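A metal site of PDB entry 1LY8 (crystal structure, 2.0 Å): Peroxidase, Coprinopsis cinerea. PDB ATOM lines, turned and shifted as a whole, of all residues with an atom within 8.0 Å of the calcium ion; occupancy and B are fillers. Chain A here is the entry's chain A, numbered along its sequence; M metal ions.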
ATOM      1  N   PRO A 129      -2.899 -25.925 -29.190  1.00  0.00           N
ATOM      2  CA  PRO A 129      -3.139 -24.649 -28.507  1.00  0.00           C
ATOM      3  C   PRO A 129      -4.004 -24.770 -27.256  1.00  0.00           C
ATOM      4  O   PRO A 129      -5.041 -25.449 -27.257  1.00  0.00           O
ATOM      5  CB  PRO A 129      -3.805 -23.804 -29.586  1.00  0.00           C
ATOM      6  CG  PRO A 129      -3.147 -24.314 -30.843  1.00  0.00           C
ATOM      7  CD  PRO A 129      -3.191 -25.806 -30.631  1.00  0.00           C
ATOM      8  N   ALA A 181     -10.854 -34.183 -19.362  1.00  0.00           N
ATOM      9  CA  ALA A 181     -10.603 -32.963 -20.111  1.00  0.00           C
ATOM     10  C   ALA A 181      -9.858 -33.328 -21.406  1.00  0.00           C
ATOM     11  O   ALA A 181      -9.838 -32.566 -22.369  1.00  0.00           O
ATOM     12  CB  ALA A 181      -9.760 -32.002 -19.277  1.00  0.00           C
ATOM     13  N   ALA A 182      -9.254 -34.508 -21.410  1.00  0.00           N
ATOM     14  CA  ALA A 182      -8.525 -34.985 -22.591  1.00  0.00           C
ATOM     15  C   ALA A 182      -9.461 -35.155 -23.776  1.00  0.00           C
ATOM     16  O   ALA A 182      -9.018 -35.169 -24.925  1.00  0.00           O
ATOM     17  CB  ALA A 182      -7.826 -36.293 -22.280  1.00  0.00           C
ATOM     18  N   HIS A 183     -10.750 -35.287 -23.518  1.00  0.00           N
ATOM     19  CA  HIS A 183     -11.705 -35.452 -24.604  1.00  0.00           C
ATOM     20  C   HIS A 183     -11.953 -34.147 -25.352  1.00  0.00           C
ATOM     21  O   HIS A 183     -12.750 -34.094 -26.282  1.00  0.00           O
ATOM     22  CB  HIS A 183     -13.020 -36.038 -24.086  1.00  0.00           C
ATOM     23  CG  HIS A 183     -12.990 -37.531 -23.955  1.00  0.00           C
ATOM     24  ND1 HIS A 183     -14.102 -38.306 -23.740  1.00  0.00           N
ATOM     25  CD2 HIS A 183     -11.941 -38.390 -24.013  1.00  0.00           C
ATOM     26  CE1 HIS A 183     -13.710 -39.592 -23.679  1.00  0.00           C
ATOM     27  NE2 HIS A 183     -12.406 -39.693 -23.843  1.00  0.00           N
ATOM     28  N   SER A 184     -11.246 -33.086 -24.937  1.00  0.00           N
ATOM     29  CA  SER A 184     -11.357 -31.796 -25.602  1.00  0.00           C
ATOM     30  C   SER A 184     -10.489 -31.837 -26.852  1.00  0.00           C
ATOM     31  O   SER A 184     -10.490 -30.904 -27.658  1.00  0.00           O
ATOM     32  CB  SER A 184     -10.887 -30.676 -24.678  1.00  0.00           C
ATOM     33  OG  SER A 184     -11.068 -29.400 -25.270  1.00  0.00           O
ATOM     34  N   LEU A 185      -9.735 -32.926 -27.001  1.00  0.00           N
ATOM     35  CA  LEU A 185      -8.852 -33.154 -28.152  1.00  0.00           C
ATOM     36  C   LEU A 185      -9.116 -34.591 -28.568  1.00  0.00           C
ATOM     37  O   LEU A 185      -8.194 -35.415 -28.658  1.00  0.00           O
ATOM     38  CB  LEU A 185      -7.377 -33.021 -27.744  1.00  0.00           C
ATOM     39  CG  LEU A 185      -6.896 -31.726 -27.076  1.00  0.00           C
ATOM     40  CD1 LEU A 185      -5.475 -31.949 -26.576  1.00  0.00           C
ATOM     41  CD2 LEU A 185      -6.958 -30.574 -28.062  1.00  0.00           C
ATOM     42  N   ALA A 186     -10.374 -34.908 -28.831  1.00  0.00           N
ATOM     43  CA  ALA A 186     -10.747 -36.279 -29.168  1.00  0.00           C
ATOM     44  C   ALA A 186     -11.761 -36.459 -30.282  1.00  0.00           C
ATOM     45  O   ALA A 186     -12.518 -35.546 -30.639  1.00  0.00           O
ATOM     46  CB  ALA A 186     -11.253 -36.970 -27.914  1.00  0.00           C
ATOM     47  N   LEU A 200     -15.340 -35.134 -30.552  1.00  0.00           N
ATOM     48  CA  LEU A 200     -16.112 -35.113 -29.317  1.00  0.00           C
ATOM     49  C   LEU A 200     -16.545 -33.700 -28.963  1.00  0.00           C
ATOM     50  O   LEU A 200     -17.549 -33.509 -28.271  1.00  0.00           O
ATOM     51  CB  LEU A 200     -15.322 -35.724 -28.160  1.00  0.00           C
ATOM     52  CG  LEU A 200     -15.303 -37.259 -28.086  1.00  0.00           C
ATOM     53  CD1 LEU A 200     -14.630 -37.833 -29.312  1.00  0.00           C
ATOM     54  CD2 LEU A 200     -14.579 -37.702 -26.839  1.00  0.00           C
ATOM     55  N   ASP A 201     -15.787 -32.693 -29.421  1.00  0.00           N
ATOM     56  CA  ASP A 201     -16.158 -31.298 -29.188  1.00  0.00           C
ATOM     57  C   ASP A 201     -15.876 -30.493 -30.458  1.00  0.00           C
ATOM     58  O   ASP A 201     -15.264 -31.005 -31.395  1.00  0.00           O
ATOM     59  CB  ASP A 201     -15.467 -30.722 -27.928  1.00  0.00           C
ATOM     60  CG  ASP A 201     -14.025 -30.260 -28.158  1.00  0.00           C
ATOM     61  OD1 ASP A 201     -13.487 -30.327 -29.286  1.00  0.00           O
ATOM     62  OD2 ASP A 201     -13.412 -29.804 -27.167  1.00  0.00           O
ATOM     63  N   SER A 202     -16.344 -29.255 -30.503  1.00  0.00           N
ATOM     64  CA  SER A 202     -16.168 -28.420 -31.689  1.00  0.00           C
ATOM     65  C   SER A 202     -14.745 -27.974 -31.981  1.00  0.00           C
ATOM     66  O   SER A 202     -14.493 -27.346 -33.017  1.00  0.00           O
ATOM     67  CB  SER A 202     -17.072 -27.181 -31.591  1.00  0.00           C
ATOM     68  OG  SER A 202     -16.709 -26.359 -30.500  1.00  0.00           O
ATOM     69  N   THR A 203     -13.811 -28.302 -31.096  1.00  0.00           N
ATOM     70  CA  THR A 203     -12.414 -27.905 -31.283  1.00  0.00           C
ATOM     71  C   THR A 203     -11.455 -29.048 -30.949  1.00  0.00           C
ATOM     72  O   THR A 203     -10.742 -28.992 -29.942  1.00  0.00           O
ATOM     73  CB  THR A 203     -12.071 -26.693 -30.399  1.00  0.00           C
ATOM     74  OG1 THR A 203     -12.480 -26.940 -29.048  1.00  0.00           O
ATOM     75  CG2 THR A 203     -12.775 -25.452 -30.915  1.00  0.00           C
ATOM     76  N   PRO A 204     -11.403 -30.079 -31.802  1.00  0.00           N
ATOM     77  CA  PRO A 204     -10.526 -31.228 -31.590  1.00  0.00           C
ATOM     78  C   PRO A 204      -9.031 -30.908 -31.560  1.00  0.00           C
ATOM     79  O   PRO A 204      -8.213 -31.752 -31.203  1.00  0.00           O
ATOM     80  CB  PRO A 204     -10.905 -32.181 -32.728  1.00  0.00           C
ATOM     81  CG  PRO A 204     -11.265 -31.234 -33.829  1.00  0.00           C
ATOM     82  CD  PRO A 204     -12.105 -30.202 -33.094  1.00  0.00           C
ATOM     83  N   GLN A 205      -8.671 -29.684 -31.938  1.00  0.00           N
ATOM     84  CA  GLN A 205      -7.265 -29.281 -31.930  1.00  0.00           C
ATOM     85  C   GLN A 205      -6.973 -28.161 -30.929  1.00  0.00           C
ATOM     86  O   GLN A 205      -5.914 -27.542 -30.968  1.00  0.00           O
ATOM     87  CB  GLN A 205      -6.803 -28.849 -33.319  1.00  0.00           C
ATOM     88  CG  GLN A 205      -6.784 -29.961 -34.340  1.00  0.00           C
ATOM     89  CD  GLN A 205      -6.192 -29.518 -35.661  1.00  0.00           C
ATOM     90  OE1 GLN A 205      -6.729 -28.643 -36.329  1.00  0.00           O
ATOM     91  NE2 GLN A 205      -5.063 -30.117 -36.027  1.00  0.00           N
ATOM     92  N   VAL A 206      -7.929 -27.894 -30.047  1.00  0.00           N
ATOM     93  CA  VAL A 206      -7.761 -26.865 -29.031  1.00  0.00           C
ATOM     94  C   VAL A 206      -8.133 -27.418 -27.665  1.00  0.00           C
ATOM     95  O   VAL A 206      -9.273 -27.820 -27.442  1.00  0.00           O
ATOM     96  CB  VAL A 206      -8.647 -25.633 -29.316  1.00  0.00           C
ATOM     97  CG1 VAL A 206      -8.499 -24.620 -28.188  1.00  0.00           C
ATOM     98  CG2 VAL A 206      -8.263 -25.004 -30.650  1.00  0.00           C
ATOM     99  N   PHE A 207      -7.171 -27.450 -26.745  1.00  0.00           N
ATOM    100  CA  PHE A 207      -7.434 -27.940 -25.402  1.00  0.00           C
ATOM    101  C   PHE A 207      -8.203 -26.845 -24.676  1.00  0.00           C
ATOM    102  O   PHE A 207      -7.600 -25.935 -24.103  1.00  0.00           O
ATOM    103  CB  PHE A 207      -6.120 -28.227 -24.675  1.00  0.00           C
ATOM    104  CG  PHE A 207      -6.312 -28.883 -23.331  1.00  0.00           C
ATOM    105  CD1 PHE A 207      -6.635 -30.237 -23.257  1.00  0.00           C
ATOM    106  CD2 PHE A 207      -6.190 -28.152 -22.159  1.00  0.00           C
ATOM    107  CE1 PHE A 207      -6.830 -30.852 -22.011  1.00  0.00           C
ATOM    108  CE2 PHE A 207      -6.388 -28.754 -20.925  1.00  0.00           C
ATOM    109  CZ  PHE A 207      -6.701 -30.113 -20.849  1.00  0.00           C
ATOM    110  N   ASP A 208      -9.528 -26.938 -24.693  1.00  0.00           N
ATOM    111  CA  ASP A 208     -10.383 -25.950 -24.056  1.00  0.00           C
ATOM    112  C   ASP A 208     -11.547 -26.597 -23.315  1.00  0.00           C
ATOM    113  O   ASP A 208     -11.649 -27.812 -23.259  1.00  0.00           O
ATOM    114  CB  ASP A 208     -10.918 -24.959 -25.095  1.00  0.00           C
ATOM    115  CG  ASP A 208     -11.487 -25.659 -26.323  1.00  0.00           C
ATOM    116  OD1 ASP A 208     -11.804 -26.865 -26.216  1.00  0.00           O
ATOM    117  OD2 ASP A 208     -11.626 -25.007 -27.375  1.00  0.00           O
ATOM    118  N   THR A 209     -12.429 -25.759 -22.774  1.00  0.00           N
ATOM    119  CA  THR A 209     -13.584 -26.239 -22.024  1.00  0.00           C
ATOM    120  C   THR A 209     -14.783 -26.577 -22.897  1.00  0.00           C
ATOM    121  O   THR A 209     -15.842 -26.951 -22.382  1.00  0.00           O
ATOM    122  CB  THR A 209     -14.072 -25.195 -20.997  1.00  0.00           C
ATOM    123  OG1 THR A 209     -14.563 -24.037 -21.697  1.00  0.00           O
ATOM    124  CG2 THR A 209     -12.934 -24.796 -20.059  1.00  0.00           C
ATOM    125  N   GLN A 210     -14.645 -26.428 -24.211  1.00  0.00           N
ATOM    126  CA  GLN A 210     -15.747 -26.708 -25.119  1.00  0.00           C
ATOM    127  C   GLN A 210     -16.362 -28.096 -24.897  1.00  0.00           C
ATOM    128  O   GLN A 210     -17.579 -28.254 -24.993  1.00  0.00           O
ATOM    129  CB  GLN A 210     -15.294 -26.573 -26.582  1.00  0.00           C
ATOM    130  CG  GLN A 210     -15.014 -25.134 -27.009  1.00  0.00           C
ATOM    131  CD  GLN A 210     -16.170 -24.200 -26.681  1.00  0.00           C
ATOM    132  OE1 GLN A 210     -16.019 -23.263 -25.879  1.00  0.00           O
ATOM    133  NE2 GLN A 210     -17.322 -24.434 -27.287  1.00  0.00           N
ATOM    134  N   PHE A 211     -15.526 -29.080 -24.611  1.00  0.00           N
ATOM    135  CA  PHE A 211     -16.020 -30.432 -24.377  1.00  0.00           C
ATOM    136  C   PHE A 211     -17.014 -30.509 -23.221  1.00  0.00           C
ATOM    137  O   PHE A 211     -18.049 -31.161 -23.327  1.00  0.00           O
ATOM    138  CB  PHE A 211     -14.859 -31.392 -24.080  1.00  0.00           C
ATOM    139  CG  PHE A 211     -15.302 -32.721 -23.527  1.00  0.00           C
ATOM    140  CD1 PHE A 211     -16.032 -33.606 -24.314  1.00  0.00           C
ATOM    141  CD2 PHE A 211     -14.977 -33.085 -22.222  1.00  0.00           C
ATOM    142  CE1 PHE A 211     -16.448 -34.837 -23.800  1.00  0.00           C
ATOM    143  CE2 PHE A 211     -15.393 -34.316 -21.709  1.00  0.00           C
ATOM    144  CZ  PHE A 211     -16.117 -35.192 -22.496  1.00  0.00           C
ATOM    145  N   TYR A 212     -16.699 -29.832 -22.117  1.00  0.00           N
ATOM    146  CA  TYR A 212     -17.574 -29.838 -20.954  1.00  0.00           C
ATOM    147  C   TYR A 212     -18.896 -29.142 -21.238  1.00  0.00           C
ATOM    148  O   TYR A 212     -19.960 -29.599 -20.804  1.00  0.00           O
ATOM    149  CB  TYR A 212     -16.873 -29.167 -19.765  1.00  0.00           C
ATOM    150  CG  TYR A 212     -15.713 -29.952 -19.227  1.00  0.00           C
ATOM    151  CD1 TYR A 212     -15.911 -31.135 -18.517  1.00  0.00           C
ATOM    152  CD2 TYR A 212     -14.409 -29.528 -19.450  1.00  0.00           C
ATOM    153  CE1 TYR A 212     -14.832 -31.878 -18.036  1.00  0.00           C
ATOM    154  CE2 TYR A 212     -13.323 -30.263 -18.980  1.00  0.00           C
ATOM    155  CZ  TYR A 212     -13.540 -31.435 -18.263  1.00  0.00           C
ATOM    156  OH  TYR A 212     -12.467 -32.152 -17.797  1.00  0.00           O
ATOM    157  N   GLU A 214     -20.394 -28.416 -24.411  1.00  0.00           N
ATOM    158  CA  GLU A 214     -21.164 -29.107 -25.433  1.00  0.00           C
ATOM    159  C   GLU A 214     -21.729 -30.469 -25.055  1.00  0.00           C
ATOM    160  O   GLU A 214     -22.761 -30.881 -25.590  1.00  0.00           O
ATOM    161  CB  GLU A 214     -20.309 -29.199 -26.698  1.00  0.00           C
ATOM    162  CG  GLU A 214     -19.878 -27.826 -27.188  1.00  0.00           C
ATOM    163  CD  GLU A 214     -18.826 -27.870 -28.269  1.00  0.00           C
ATOM    164  OE1 GLU A 214     -18.394 -26.793 -28.709  1.00  0.00           O
ATOM    165  OE2 GLU A 214     -18.431 -28.988 -28.667  1.00  0.00           O
ATOM    166  N   ASN A 265     -10.627 -21.990 -18.751  1.00  0.00           N
ATOM    167  CA  ASN A 265      -9.633 -22.849 -19.376  1.00  0.00           C
ATOM    168  C   ASN A 265      -8.413 -23.005 -18.465  1.00  0.00           C
ATOM    169  O   ASN A 265      -7.776 -24.052 -18.442  1.00  0.00           O
ATOM    170  CB  ASN A 265      -9.194 -22.298 -20.732  1.00  0.00           C
ATOM    171  CG  ASN A 265     -10.224 -22.537 -21.819  1.00  0.00           C
ATOM    172  OD1 ASN A 265     -10.690 -23.663 -22.009  1.00  0.00           O
ATOM    173  ND2 ASN A 265     -10.579 -21.480 -22.548  1.00  0.00           N
ATOM    174  N   MET A 268      -9.174 -25.527 -15.730  1.00  0.00           N
ATOM    175  CA  MET A 268      -9.205 -26.832 -16.355  1.00  0.00           C
ATOM    176  C   MET A 268      -7.785 -27.344 -16.550  1.00  0.00           C
ATOM    177  O   MET A 268      -7.466 -28.495 -16.231  1.00  0.00           O
ATOM    178  CB  MET A 268      -9.914 -26.759 -17.704  1.00  0.00           C
ATOM    179  CG  MET A 268      -9.928 -28.080 -18.457  1.00  0.00           C
ATOM    180  SD  MET A 268     -10.724 -27.950 -20.070  1.00  0.00           S
ATOM    181  CE  MET A 268      -9.389 -27.261 -21.017  1.00  0.00           C
ATOM    182  N   ASN A 302      -4.316 -20.318 -25.792  1.00  0.00           N
ATOM    183  CA  ASN A 302      -5.658 -20.247 -26.353  1.00  0.00           C
ATOM    184  C   ASN A 302      -6.301 -18.930 -25.913  1.00  0.00           C
ATOM    185  O   ASN A 302      -6.580 -18.730 -24.726  1.00  0.00           O
ATOM    186  CB  ASN A 302      -6.507 -21.418 -25.835  1.00  0.00           C
ATOM    187  CG  ASN A 302      -7.915 -21.402 -26.387  1.00  0.00           C
ATOM    188  OD1 ASN A 302      -8.822 -22.008 -25.820  1.00  0.00           O
ATOM    189  ND2 ASN A 302      -8.110 -20.710 -27.504  1.00  0.00           N
HETATM  190 CA    CA M   1     -11.452 -28.776 -27.655  1.00  0.00          CA
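OD2 of Asp 201 lies close to N of Phe 211 (3.4 Å).
The calcium ion is bound by OD2 of Asp 201, O of Ser 184, O of Val 206, O of Thr 203, OD1 of Asp 208, OG of Ser 184 and OG1 of Thr 203.
The calcium ion has seven donor atoms within binding distance.
Slightly farther from the calcium ion lies OD1 of Asp 201 (3.0 Å).
Five residues have an atom within 4 Å of the calcium ion: Ser 184, Asp 201, Thr 203, Val 206 and Asp 208.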
